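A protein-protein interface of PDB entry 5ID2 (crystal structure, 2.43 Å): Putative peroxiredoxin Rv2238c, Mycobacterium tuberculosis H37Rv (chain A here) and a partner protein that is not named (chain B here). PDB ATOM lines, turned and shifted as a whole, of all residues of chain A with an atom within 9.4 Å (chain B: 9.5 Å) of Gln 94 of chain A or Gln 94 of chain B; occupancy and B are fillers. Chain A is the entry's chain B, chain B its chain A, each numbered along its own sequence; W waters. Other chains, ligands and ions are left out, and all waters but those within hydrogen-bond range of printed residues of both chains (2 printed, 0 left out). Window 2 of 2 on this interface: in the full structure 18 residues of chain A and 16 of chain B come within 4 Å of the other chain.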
ATOM      1  N   PHE A  52     -11.297  24.006  23.159  1.00  0.00           N
ATOM      2  CA  PHE A  52     -11.479  25.459  23.078  1.00  0.00           C
ATOM      3  C   PHE A  52     -10.212  26.260  23.346  1.00  0.00           C
ATOM      4  O   PHE A  52     -10.278  27.359  23.891  1.00  0.00           O
ATOM      5  CB  PHE A  52     -12.563  25.939  24.042  1.00  0.00           C
ATOM      6  CG  PHE A  52     -13.861  25.211  23.910  1.00  0.00           C
ATOM      7  CD1 PHE A  52     -14.341  24.439  24.955  1.00  0.00           C
ATOM      8  CD2 PHE A  52     -14.626  25.331  22.759  1.00  0.00           C
ATOM      9  CE1 PHE A  52     -15.555  23.782  24.844  1.00  0.00           C
ATOM     10  CE2 PHE A  52     -15.845  24.683  22.646  1.00  0.00           C
ATOM     11  CZ  PHE A  52     -16.305  23.902  23.687  1.00  0.00           C
ATOM     12  N   GLN A  57      -7.257  23.802  18.714  1.00  0.00           N
ATOM     13  CA  GLN A  57      -8.163  24.118  17.599  1.00  0.00           C
ATOM     14  C   GLN A  57      -7.445  23.952  16.263  1.00  0.00           C
ATOM     15  O   GLN A  57      -7.945  23.285  15.368  1.00  0.00           O
ATOM     16  CB  GLN A  57      -8.698  25.555  17.700  1.00  0.00           C
ATOM     17  CG  GLN A  57      -9.807  25.886  16.705  1.00  0.00           C
ATOM     18  CD  GLN A  57     -11.145  25.297  17.105  1.00  0.00           C
ATOM     19  OE1 GLN A  57     -11.658  25.596  18.175  1.00  0.00           O
ATOM     20  NE2 GLN A  57     -11.701  24.432  16.263  1.00  0.00           N
ATOM     21  N   ASP A  61      -8.251  21.097  13.632  1.00  0.00           N
ATOM     22  CA  ASP A  61      -8.700  21.669  12.354  1.00  0.00           C
ATOM     23  C   ASP A  61      -7.909  21.056  11.198  1.00  0.00           C
ATOM     24  O   ASP A  61      -8.480  20.684  10.174  1.00  0.00           O
ATOM     25  CB  ASP A  61      -8.548  23.191  12.323  1.00  0.00           C
ATOM     26  CG  ASP A  61      -9.647  23.916  13.082  1.00  0.00           C
ATOM     27  OD1 ASP A  61     -10.580  23.275  13.593  1.00  0.00           O
ATOM     28  OD2 ASP A  61      -9.569  25.154  13.171  1.00  0.00           O
ATOM     29  N   ARG A  64      -9.119  17.562  10.790  1.00  0.00           N
ATOM     30  CA  ARG A  64     -10.399  17.660  10.084  1.00  0.00           C
ATOM     31  C   ARG A  64     -10.216  17.923   8.585  1.00  0.00           C
ATOM     32  O   ARG A  64     -10.825  17.252   7.751  1.00  0.00           O
ATOM     33  CB  ARG A  64     -11.240  18.784  10.695  1.00  0.00           C
ATOM     34  CG  ARG A  64     -12.547  19.102   9.976  1.00  0.00           C
ATOM     35  CD  ARG A  64     -13.032  20.492  10.360  1.00  0.00           C
ATOM     36  NE  ARG A  64     -12.108  21.510   9.871  1.00  0.00           N
ATOM     37  CZ  ARG A  64     -12.068  22.776  10.276  1.00  0.00           C
ATOM     38  NH1 ARG A  64     -12.898  23.224  11.207  1.00  0.00           N
ATOM     39  NH2 ARG A  64     -11.168  23.594   9.754  1.00  0.00           N
ATOM     40  N   PRO A  86     -19.996  16.207  26.930  1.00  0.00           N
ATOM     41  CA  PRO A  86     -20.716  17.412  26.508  1.00  0.00           C
ATOM     42  C   PRO A  86     -19.797  18.523  26.011  1.00  0.00           C
ATOM     43  O   PRO A  86     -20.149  19.245  25.077  1.00  0.00           O
ATOM     44  CB  PRO A  86     -21.447  17.849  27.783  1.00  0.00           C
ATOM     45  CG  PRO A  86     -21.592  16.599  28.564  1.00  0.00           C
ATOM     46  CD  PRO A  86     -20.322  15.846  28.317  1.00  0.00           C
ATOM     47  N   THR A  87     -18.628  18.652  26.628  1.00  0.00           N
ATOM     48  CA  THR A  87     -17.640  19.621  26.173  1.00  0.00           C
ATOM     49  C   THR A  87     -17.181  19.291  24.749  1.00  0.00           C
ATOM     50  O   THR A  87     -17.138  20.166  23.892  1.00  0.00           O
ATOM     51  CB  THR A  87     -16.432  19.675  27.127  1.00  0.00           C
ATOM     52  OG1 THR A  87     -16.842  20.263  28.366  1.00  0.00           O
ATOM     53  CG2 THR A  87     -15.294  20.493  26.539  1.00  0.00           C
ATOM     54  N   HIS A  88     -16.843  18.028  24.512  1.00  0.00           N
ATOM     55  CA  HIS A  88     -16.375  17.594  23.206  1.00  0.00           C
ATOM     56  C   HIS A  88     -17.467  17.673  22.139  1.00  0.00           C
ATOM     57  O   HIS A  88     -17.176  17.967  20.975  1.00  0.00           O
ATOM     58  CB  HIS A  88     -15.798  16.178  23.282  1.00  0.00           C
ATOM     59  CG  HIS A  88     -14.510  16.092  24.044  1.00  0.00           C
ATOM     60  ND1 HIS A  88     -14.100  14.948  24.693  1.00  0.00           N
ATOM     61  CD2 HIS A  88     -13.547  17.016  24.269  1.00  0.00           C
ATOM     62  CE1 HIS A  88     -12.930  15.163  25.267  1.00  0.00           C
ATOM     63  NE2 HIS A  88     -12.577  16.415  25.034  1.00  0.00           N
ATOM     64  N   LYS A  89     -18.712  17.417  22.532  1.00  0.00           N
ATOM     65  CA  LYS A  89     -19.844  17.477  21.607  1.00  0.00           C
ATOM     66  C   LYS A  89     -20.027  18.883  21.050  1.00  0.00           C
ATOM     67  O   LYS A  89     -20.090  19.068  19.831  1.00  0.00           O
ATOM     68  CB  LYS A  89     -21.125  17.009  22.309  1.00  0.00           C
ATOM     69  CG  LYS A  89     -22.368  16.930  21.428  1.00  0.00           C
ATOM     70  CD  LYS A  89     -22.143  16.111  20.161  1.00  0.00           C
ATOM     71  CE  LYS A  89     -23.415  15.989  19.330  1.00  0.00           C
ATOM     72  NZ  LYS A  89     -23.146  15.355  18.004  1.00  0.00           N
ATOM     73  N   ILE A  90     -20.089  19.873  21.937  1.00  0.00           N
ATOM     74  CA  ILE A  90     -20.261  21.258  21.511  1.00  0.00           C
ATOM     75  C   ILE A  90     -19.074  21.723  20.667  1.00  0.00           C
ATOM     76  O   ILE A  90     -19.250  22.361  19.628  1.00  0.00           O
ATOM     77  CB  ILE A  90     -20.448  22.211  22.706  1.00  0.00           C
ATOM     78  CG1 ILE A  90     -21.731  21.873  23.474  1.00  0.00           C
ATOM     79  CG2 ILE A  90     -20.512  23.661  22.238  1.00  0.00           C
ATOM     80  CD1 ILE A  90     -23.008  21.911  22.648  1.00  0.00           C
ATOM     81  N   TRP A  91     -17.867  21.389  21.103  1.00  0.00           N
ATOM     82  CA  TRP A  91     -16.677  21.774  20.356  1.00  0.00           C
ATOM     83  C   TRP A  91     -16.666  21.139  18.964  1.00  0.00           C
ATOM     84  O   TRP A  91     -16.356  21.807  17.980  1.00  0.00           O
ATOM     85  CB  TRP A  91     -15.407  21.407  21.118  1.00  0.00           C
ATOM     86  CG  TRP A  91     -14.186  22.098  20.605  1.00  0.00           C
ATOM     87  CD1 TRP A  91     -14.109  23.360  20.117  1.00  0.00           C
ATOM     88  CD2 TRP A  91     -12.848  21.573  20.572  1.00  0.00           C
ATOM     89  NE1 TRP A  91     -12.820  23.652  19.760  1.00  0.00           N
ATOM     90  CE2 TRP A  91     -12.023  22.574  20.026  1.00  0.00           C
ATOM     91  CE3 TRP A  91     -12.274  20.351  20.941  1.00  0.00           C
ATOM     92  CZ2 TRP A  91     -10.652  22.402  19.844  1.00  0.00           C
ATOM     93  CZ3 TRP A  91     -10.913  20.175  20.757  1.00  0.00           C
ATOM     94  CH2 TRP A  91     -10.114  21.199  20.210  1.00  0.00           C
ATOM     95  N   ALA A  92     -17.021  19.861  18.896  1.00  0.00           N
ATOM     96  CA  ALA A  92     -17.014  19.113  17.644  1.00  0.00           C
ATOM     97  C   ALA A  92     -18.069  19.627  16.670  1.00  0.00           C
ATOM     98  O   ALA A  92     -17.791  19.793  15.482  1.00  0.00           O
ATOM     99  CB  ALA A  92     -17.219  17.628  17.909  1.00  0.00           C
ATOM    100  N   THR A  93     -19.274  19.868  17.177  1.00  0.00           N
ATOM    101  CA  THR A  93     -20.364  20.424  16.368  1.00  0.00           C
ATOM    102  C   THR A  93     -19.975  21.778  15.792  1.00  0.00           C
ATOM    103  O   THR A  93     -20.166  22.023  14.604  1.00  0.00           O
ATOM    104  CB  THR A  93     -21.662  20.600  17.201  1.00  0.00           C
ATOM    105  OG1 THR A  93     -22.094  19.327  17.684  1.00  0.00           O
ATOM    106  CG2 THR A  93     -22.782  21.209  16.360  1.00  0.00           C
ATOM    107  N   GLN A  94     -19.430  22.649  16.639  1.00  0.00           N
ATOM    108  CA  GLN A  94     -19.059  24.002  16.213  1.00  0.00           C
ATOM    109  C   GLN A  94     -17.821  24.042  15.320  1.00  0.00           C
ATOM    110  O   GLN A  94     -17.656  24.982  14.560  1.00  0.00           O
ATOM    111  CB  GLN A  94     -18.850  24.910  17.423  1.00  0.00           C
ATOM    112  CG  GLN A  94     -20.133  25.195  18.189  1.00  0.00           C
ATOM    113  CD  GLN A  94     -19.920  26.080  19.401  1.00  0.00           C
ATOM    114  OE1 GLN A  94     -18.807  26.513  19.686  1.00  0.00           O
ATOM    115  NE2 GLN A  94     -20.998  26.350  20.128  1.00  0.00           N
ATOM    116  N   SER A  95     -16.957  23.031  15.424  1.00  0.00           N
ATOM    117  CA  SER A  95     -15.740  22.960  14.624  1.00  0.00           C
ATOM    118  C   SER A  95     -15.871  22.047  13.399  1.00  0.00           C
ATOM    119  O   SER A  95     -14.986  22.025  12.542  1.00  0.00           O
ATOM    120  CB  SER A  95     -14.578  22.467  15.483  1.00  0.00           C
ATOM    121  OG  SER A  95     -14.387  23.280  16.633  1.00  0.00           O
ATOM    122  N   GLY A  96     -16.961  21.285  13.324  1.00  0.00           N
ATOM    123  CA  GLY A  96     -17.133  20.291  12.277  1.00  0.00           C
ATOM    124  C   GLY A  96     -16.198  19.095  12.400  1.00  0.00           C
ATOM    125  O   GLY A  96     -15.680  18.600  11.393  1.00  0.00           O
ATOM    126  N   PHE A  97     -15.954  18.639  13.631  1.00  0.00           N
ATOM    127  CA  PHE A  97     -15.172  17.425  13.865  1.00  0.00           C
ATOM    128  C   PHE A  97     -16.121  16.235  13.846  1.00  0.00           C
ATOM    129  O   PHE A  97     -17.029  16.157  14.676  1.00  0.00           O
ATOM    130  CB  PHE A  97     -14.442  17.468  15.217  1.00  0.00           C
ATOM    131  CG  PHE A  97     -13.475  18.618  15.378  1.00  0.00           C
ATOM    132  CD1 PHE A  97     -12.793  19.158  14.290  1.00  0.00           C
ATOM    133  CD2 PHE A  97     -13.213  19.137  16.645  1.00  0.00           C
ATOM    134  CE1 PHE A  97     -11.892  20.200  14.462  1.00  0.00           C
ATOM    135  CE2 PHE A  97     -12.307  20.177  16.816  1.00  0.00           C
ATOM    136  CZ  PHE A  97     -11.651  20.712  15.722  1.00  0.00           C
ATOM    137  N   THR A  98     -15.919  15.320  12.897  1.00  0.00           N
ATOM    138  CA  THR A  98     -16.757  14.112  12.771  1.00  0.00           C
ATOM    139  C   THR A  98     -16.025  12.853  13.216  1.00  0.00           C
ATOM    140  O   THR A  98     -16.616  11.783  13.277  1.00  0.00           O
ATOM    141  CB  THR A  98     -17.235  13.914  11.321  1.00  0.00           C
ATOM    142  OG1 THR A  98     -16.098  13.793  10.450  1.00  0.00           O
ATOM    143  CG2 THR A  98     -18.092  15.096  10.886  1.00  0.00           C
ATOM    144  N   LEU A 101     -13.846  12.176  19.475  1.00  0.00           N
ATOM    145  CA  LEU A 101     -13.159  12.814  20.590  1.00  0.00           C
ATOM    146  C   LEU A 101     -13.538  12.058  21.852  1.00  0.00           C
ATOM    147  O   LEU A 101     -14.716  12.004  22.196  1.00  0.00           O
ATOM    148  CB  LEU A 101     -13.584  14.271  20.750  1.00  0.00           C
ATOM    149  CG  LEU A 101     -12.927  15.277  19.825  1.00  0.00           C
ATOM    150  CD1 LEU A 101     -13.420  15.114  18.398  1.00  0.00           C
ATOM    151  CD2 LEU A 101     -13.222  16.681  20.327  1.00  0.00           C
ATOM    152  N   PHE B  52     -22.567  23.320  29.500  1.00  0.00           N
ATOM    153  CA  PHE B  52     -23.251  22.888  28.276  1.00  0.00           C
ATOM    154  C   PHE B  52     -24.313  21.816  28.516  1.00  0.00           C
ATOM    155  O   PHE B  52     -24.529  20.966  27.662  1.00  0.00           O
ATOM    156  CB  PHE B  52     -22.258  22.370  27.228  1.00  0.00           C
ATOM    157  CG  PHE B  52     -21.137  23.320  26.918  1.00  0.00           C
ATOM    158  CD1 PHE B  52     -19.822  22.992  27.225  1.00  0.00           C
ATOM    159  CD2 PHE B  52     -21.391  24.531  26.300  1.00  0.00           C
ATOM    160  CE1 PHE B  52     -18.788  23.867  26.931  1.00  0.00           C
ATOM    161  CE2 PHE B  52     -20.359  25.403  26.001  1.00  0.00           C
ATOM    162  CZ  PHE B  52     -19.057  25.075  26.325  1.00  0.00           C
ATOM    163  N   GLN B  57     -27.548  25.295  32.210  1.00  0.00           N
ATOM    164  CA  GLN B  57     -27.802  26.458  31.365  1.00  0.00           C
ATOM    165  C   GLN B  57     -28.922  27.301  31.957  1.00  0.00           C
ATOM    166  O   GLN B  57     -28.787  28.517  32.088  1.00  0.00           O
ATOM    167  CB  GLN B  57     -28.176  26.027  29.943  1.00  0.00           C
ATOM    168  CG  GLN B  57     -28.236  27.170  28.941  1.00  0.00           C
ATOM    169  CD  GLN B  57     -26.853  27.646  28.526  1.00  0.00           C
ATOM    170  OE1 GLN B  57     -26.074  26.883  27.966  1.00  0.00           O
ATOM    171  NE2 GLN B  57     -26.550  28.911  28.785  1.00  0.00           N
ATOM    172  N   ASP B  61     -28.441  30.947  33.471  1.00  0.00           N
ATOM    173  CA  ASP B  61     -29.221  31.947  32.733  1.00  0.00           C
ATOM    174  C   ASP B  61     -30.039  32.809  33.707  1.00  0.00           C
ATOM    175  O   ASP B  61     -30.094  34.028  33.552  1.00  0.00           O
ATOM    176  CB  ASP B  61     -30.149  31.286  31.703  1.00  0.00           C
ATOM    177  CG  ASP B  61     -29.422  30.823  30.451  1.00  0.00           C
ATOM    178  OD1 ASP B  61     -28.202  31.067  30.308  1.00  0.00           O
ATOM    179  OD2 ASP B  61     -30.086  30.221  29.582  1.00  0.00           O
ATOM    180  N   ARG B  64     -27.631  35.071  35.420  1.00  0.00           N
ATOM    181  CA  ARG B  64     -27.320  36.137  34.473  1.00  0.00           C
ATOM    182  C   ARG B  64     -28.452  37.176  34.379  1.00  0.00           C
ATOM    183  O   ARG B  64     -28.199  38.389  34.409  1.00  0.00           O
ATOM    184  CB  ARG B  64     -27.071  35.529  33.096  1.00  0.00           C
ATOM    185  CG  ARG B  64     -26.867  36.527  31.965  1.00  0.00           C
ATOM    186  CD  ARG B  64     -27.095  35.844  30.634  1.00  0.00           C
ATOM    187  NE  ARG B  64     -28.489  35.431  30.506  1.00  0.00           N
ATOM    188  CZ  ARG B  64     -28.951  34.564  29.615  1.00  0.00           C
ATOM    189  NH1 ARG B  64     -28.132  33.975  28.745  1.00  0.00           N
ATOM    190  NH2 ARG B  64     -30.248  34.286  29.594  1.00  0.00           N
ATOM    191  N   PRO B  86     -10.863  27.142  29.793  1.00  0.00           N
ATOM    192  CA  PRO B  86     -11.291  27.306  28.405  1.00  0.00           C
ATOM    193  C   PRO B  86     -12.736  26.878  28.172  1.00  0.00           C
ATOM    194  O   PRO B  86     -13.435  27.479  27.355  1.00  0.00           O
ATOM    195  CB  PRO B  86     -10.325  26.405  27.629  1.00  0.00           C
ATOM    196  CG  PRO B  86      -9.118  26.331  28.489  1.00  0.00           C
ATOM    197  CD  PRO B  86      -9.665  26.295  29.890  1.00  0.00           C
ATOM    198  N   THR B  87     -13.167  25.830  28.858  1.00  0.00           N
ATOM    199  CA  THR B  87     -14.555  25.370  28.757  1.00  0.00           C
ATOM    200  C   THR B  87     -15.506  26.444  29.263  1.00  0.00           C
ATOM    201  O   THR B  87     -16.473  26.775  28.594  1.00  0.00           O
ATOM    202  CB  THR B  87     -14.769  24.061  29.540  1.00  0.00           C
ATOM    203  OG1 THR B  87     -14.079  22.999  28.865  1.00  0.00           O
ATOM    204  CG2 THR B  87     -16.241  23.713  29.643  1.00  0.00           C
ATOM    205  N   HIS B  88     -15.195  27.002  30.432  1.00  0.00           N
ATOM    206  CA  HIS B  88     -16.007  28.052  31.019  1.00  0.00           C
ATOM    207  C   HIS B  88     -15.980  29.356  30.209  1.00  0.00           C
ATOM    208  O   HIS B  88     -16.989  30.043  30.123  1.00  0.00           O
ATOM    209  CB  HIS B  88     -15.586  28.319  32.460  1.00  0.00           C
ATOM    210  CG  HIS B  88     -15.913  27.202  33.403  1.00  0.00           C
ATOM    211  ND1 HIS B  88     -15.206  26.974  34.566  1.00  0.00           N
ATOM    212  CD2 HIS B  88     -16.864  26.244  33.349  1.00  0.00           C
ATOM    213  CE1 HIS B  88     -15.711  25.923  35.186  1.00  0.00           C
ATOM    214  NE2 HIS B  88     -16.722  25.465  34.471  1.00  0.00           N
ATOM    215  N   LYS B  89     -14.842  29.674  29.598  1.00  0.00           N
ATOM    216  CA  LYS B  89     -14.718  30.873  28.771  1.00  0.00           C
ATOM    217  C   LYS B  89     -15.669  30.836  27.567  1.00  0.00           C
ATOM    218  O   LYS B  89     -16.433  31.775  27.341  1.00  0.00           O
ATOM    219  CB  LYS B  89     -13.268  31.040  28.294  1.00  0.00           C
ATOM    220  CG  LYS B  89     -12.965  32.312  27.501  1.00  0.00           C
ATOM    221  CD  LYS B  89     -13.402  33.571  28.236  1.00  0.00           C
ATOM    222  CE  LYS B  89     -13.035  34.836  27.468  1.00  0.00           C
ATOM    223  NZ  LYS B  89     -13.633  36.046  28.107  1.00  0.00           N
ATOM    224  N   ILE B  90     -15.627  29.748  26.807  1.00  0.00           N
ATOM    225  CA  ILE B  90     -16.494  29.609  25.642  1.00  0.00           C
ATOM    226  C   ILE B  90     -17.969  29.595  26.052  1.00  0.00           C
ATOM    227  O   ILE B  90     -18.802  30.244  25.411  1.00  0.00           O
ATOM    228  CB  ILE B  90     -16.171  28.337  24.837  1.00  0.00           C
ATOM    229  CG1 ILE B  90     -14.750  28.412  24.270  1.00  0.00           C
ATOM    230  CG2 ILE B  90     -17.152  28.153  23.690  1.00  0.00           C
ATOM    231  CD1 ILE B  90     -14.463  29.606  23.377  1.00  0.00           C
ATOM    232  N   TRP B  91     -18.291  28.853  27.107  1.00  0.00           N
ATOM    233  CA  TRP B  91     -19.670  28.786  27.571  1.00  0.00           C
ATOM    234  C   TRP B  91     -20.161  30.159  28.009  1.00  0.00           C
ATOM    235  O   TRP B  91     -21.277  30.555  27.678  1.00  0.00           O
ATOM    236  CB  TRP B  91     -19.823  27.783  28.708  1.00  0.00           C
ATOM    237  CG  TRP B  91     -21.248  27.390  28.976  1.00  0.00           C
ATOM    238  CD1 TRP B  91     -22.244  27.243  28.057  1.00  0.00           C
ATOM    239  CD2 TRP B  91     -21.823  27.065  30.245  1.00  0.00           C
ATOM    240  NE1 TRP B  91     -23.407  26.858  28.675  1.00  0.00           N
ATOM    241  CE2 TRP B  91     -23.175  26.740  30.019  1.00  0.00           C
ATOM    242  CE3 TRP B  91     -21.327  27.026  31.550  1.00  0.00           C
ATOM    243  CZ2 TRP B  91     -24.041  26.372  31.052  1.00  0.00           C
ATOM    244  CZ3 TRP B  91     -22.187  26.662  32.578  1.00  0.00           C
ATOM    245  CH2 TRP B  91     -23.529  26.335  32.320  1.00  0.00           C
ATOM    246  N   ALA B  92     -19.306  30.882  28.722  1.00  0.00           N
ATOM    247  CA  ALA B  92     -19.648  32.200  29.252  1.00  0.00           C
ATOM    248  C   ALA B  92     -19.840  33.224  28.145  1.00  0.00           C
ATOM    249  O   ALA B  92     -20.799  33.987  28.159  1.00  0.00           O
ATOM    250  CB  ALA B  92     -18.579  32.669  30.238  1.00  0.00           C
ATOM    251  N   THR B  93     -18.919  33.231  27.185  1.00  0.00           N
ATOM    252  CA  THR B  93     -19.009  34.125  26.031  1.00  0.00           C
ATOM    253  C   THR B  93     -20.292  33.877  25.244  1.00  0.00           C
ATOM    254  O   THR B  93     -21.002  34.823  24.897  1.00  0.00           O
ATOM    255  CB  THR B  93     -17.801  33.956  25.092  1.00  0.00           C
ATOM    256  OG1 THR B  93     -16.591  34.279  25.796  1.00  0.00           O
ATOM    257  CG2 THR B  93     -17.924  34.870  23.868  1.00  0.00           C
ATOM    258  N   GLN B  94     -20.591  32.608  24.970  1.00  0.00           N
ATOM    259  CA  GLN B  94     -21.778  32.246  24.187  1.00  0.00           C
ATOM    260  C   GLN B  94     -23.090  32.418  24.945  1.00  0.00           C
ATOM    261  O   GLN B  94     -24.128  32.584  24.327  1.00  0.00           O
ATOM    262  CB  GLN B  94     -21.667  30.808  23.677  1.00  0.00           C
ATOM    263  CG  GLN B  94     -20.564  30.632  22.646  1.00  0.00           C
ATOM    264  CD  GLN B  94     -20.425  29.206  22.160  1.00  0.00           C
ATOM    265  OE1 GLN B  94     -21.181  28.319  22.563  1.00  0.00           O
ATOM    266  NE2 GLN B  94     -19.457  28.981  21.283  1.00  0.00           N
ATOM    267  N   SER B  95     -23.046  32.365  26.274  1.00  0.00           N
ATOM    268  CA  SER B  95     -24.246  32.531  27.107  1.00  0.00           C
ATOM    269  C   SER B  95     -24.401  33.949  27.655  1.00  0.00           C
ATOM    270  O   SER B  95     -25.431  34.279  28.251  1.00  0.00           O
ATOM    271  CB  SER B  95     -24.202  31.549  28.283  1.00  0.00           C
ATOM    272  OG  SER B  95     -24.067  30.212  27.839  1.00  0.00           O
ATOM    273  N   GLY B  96     -23.369  34.772  27.504  1.00  0.00           N
ATOM    274  CA  GLY B  96     -23.359  36.099  28.110  1.00  0.00           C
ATOM    275  C   GLY B  96     -23.232  36.088  29.628  1.00  0.00           C
ATOM    276  O   GLY B  96     -23.853  36.908  30.308  1.00  0.00           O
ATOM    277  N   PHE B  97     -22.414  35.179  30.159  1.00  0.00           N
ATOM    278  CA  PHE B  97     -22.092  35.169  31.579  1.00  0.00           C
ATOM    279  C   PHE B  97     -20.872  36.068  31.814  1.00  0.00           C
ATOM    280  O   PHE B  97     -19.787  35.794  31.313  1.00  0.00           O
ATOM    281  CB  PHE B  97     -21.784  33.746  32.087  1.00  0.00           C
ATOM    282  CG  PHE B  97     -22.899  32.740  31.882  1.00  0.00           C
ATOM    283  CD1 PHE B  97     -24.236  33.116  31.904  1.00  0.00           C
ATOM    284  CD2 PHE B  97     -22.596  31.390  31.716  1.00  0.00           C
ATOM    285  CE1 PHE B  97     -25.247  32.173  31.737  1.00  0.00           C
ATOM    286  CE2 PHE B  97     -23.604  30.442  31.552  1.00  0.00           C
ATOM    287  CZ  PHE B  97     -24.931  30.835  31.566  1.00  0.00           C
ATOM    288  N   THR B  98     -21.041  37.123  32.602  1.00  0.00           N
ATOM    289  CA  THR B  98     -19.936  38.030  32.933  1.00  0.00           C
ATOM    290  C   THR B  98     -19.458  37.858  34.382  1.00  0.00           C
ATOM    291  O   THR B  98     -18.476  38.478  34.792  1.00  0.00           O
ATOM    292  CB  THR B  98     -20.346  39.497  32.704  1.00  0.00           C
ATOM    293  OG1 THR B  98     -21.473  39.805  33.528  1.00  0.00           O
ATOM    294  CG2 THR B  98     -20.701  39.727  31.239  1.00  0.00           C
ATOM    295  N   LEU B 101     -16.907  32.173  36.610  1.00  0.00           N
ATOM    296  CA  LEU B 101     -17.017  30.726  36.629  1.00  0.00           C
ATOM    297  C   LEU B 101     -15.646  30.186  37.006  1.00  0.00           C
ATOM    298  O   LEU B 101     -14.683  30.418  36.273  1.00  0.00           O
ATOM    299  CB  LEU B 101     -17.418  30.186  35.261  1.00  0.00           C
ATOM    300  CG  LEU B 101     -18.897  30.248  34.892  1.00  0.00           C
ATOM    301  CD1 LEU B 101     -19.330  31.684  34.639  1.00  0.00           C
ATOM    302  CD2 LEU B 101     -19.159  29.397  33.664  1.00  0.00           C
HETATM  303  O   HOH W   1     -11.833  29.248  25.558  1.00  0.00           O
HETATM  304  O   HOH W   2     -14.698  20.823  30.012  1.00  0.00           O
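Printed residues of chain B within 4 Å of Phe 52 of chain A: Phe 52, Pro 86, Thr 87 and Ile 90. Printed residues of chain B within 4 Å of Thr 87 of chain A: Thr 87 (3.6 Å). Of the printed residues of chain B, Ile 90 of chain A touches Phe 52. No residue of chain B comes within 4 Å of Thr 93 of chain A. Gln 94 of chain A touches just one residue of chain B: Gln 94. Ser 95 of chain A touches none of the printed residues of chain B. Printed residues of chain A within 4 Å of Phe 52 of chain B: Phe 52 (3.8 Å) and Ile 90 (3.8 Å). Of the printed residues of chain A, Pro 86 of chain B touches Phe 52. His 88 of chain B touches none of the printed residues of chain A. No residue of chain A comes within 4 Å of Thr 93 of chain B. Gln 94 of chain B touches just one residue of chain A: Gln 94 (3.0 Å). No residue of chain A comes within 4 Å of Ser 95 of chain B. The nearest residue of chain B that does not touch Gln 94 of chain A is Ile 90 of chain B (4.6 Å). The nearest residue of chain A that does not touch Gln 94 of chain B is Ile 90 of chain A (4.7 Å). The nearest printed residue of chain A that does not touch Pro 86 of chain B is Thr 87 of chain A (7.1 Å).
Water W2 bridges OG1 of Thr 87 of chain B (2.5 Å) and OG1 of Thr 87 of chain A (2.8 Å). Water W1 lies within hydrogen-bond range of O of Phe 52 of chain A (3.0 Å) and O of Pro 86 of chain B (3.0 Å).
OE1 of Gln 94 of chain A is in hydrogen-bond range of NE2 of Gln 94 of chain B (3.0 Å).
Hydrophobic or aromatic side chains of chain B that line the printed part of chain A: Phe 52, Pro 86 and Ile 90. Along chain B the printed residues that touch a printed residue of chain A span positions 52 to 94. Of the 18 printed residues of chain A, 4 touch a printed residue of chain B. Hydrophobic or aromatic side chains of chain A that line the printed part of chain B: Phe 52 and Ile 90. Among the printed residues, 7 pairs touch across the chains. Among the printed residues, no Asp or Glu carboxylate lies within 4 Å of a Lys or Arg side-chain nitrogen of the other chain.
Among the printed residues, merely in contact across the chains: Phe 52 of chain A with Ile 90 of chain B, Thr 87 of chain A with Thr 87 of chain B, Phe 52 of chain A with Pro 86 of chain B, Ile 90 of chain A with Phe 52 of chain B, Phe 52 of chain A with Phe 52 of chain B and Phe 52 of chain A with Thr 87 of chain B.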
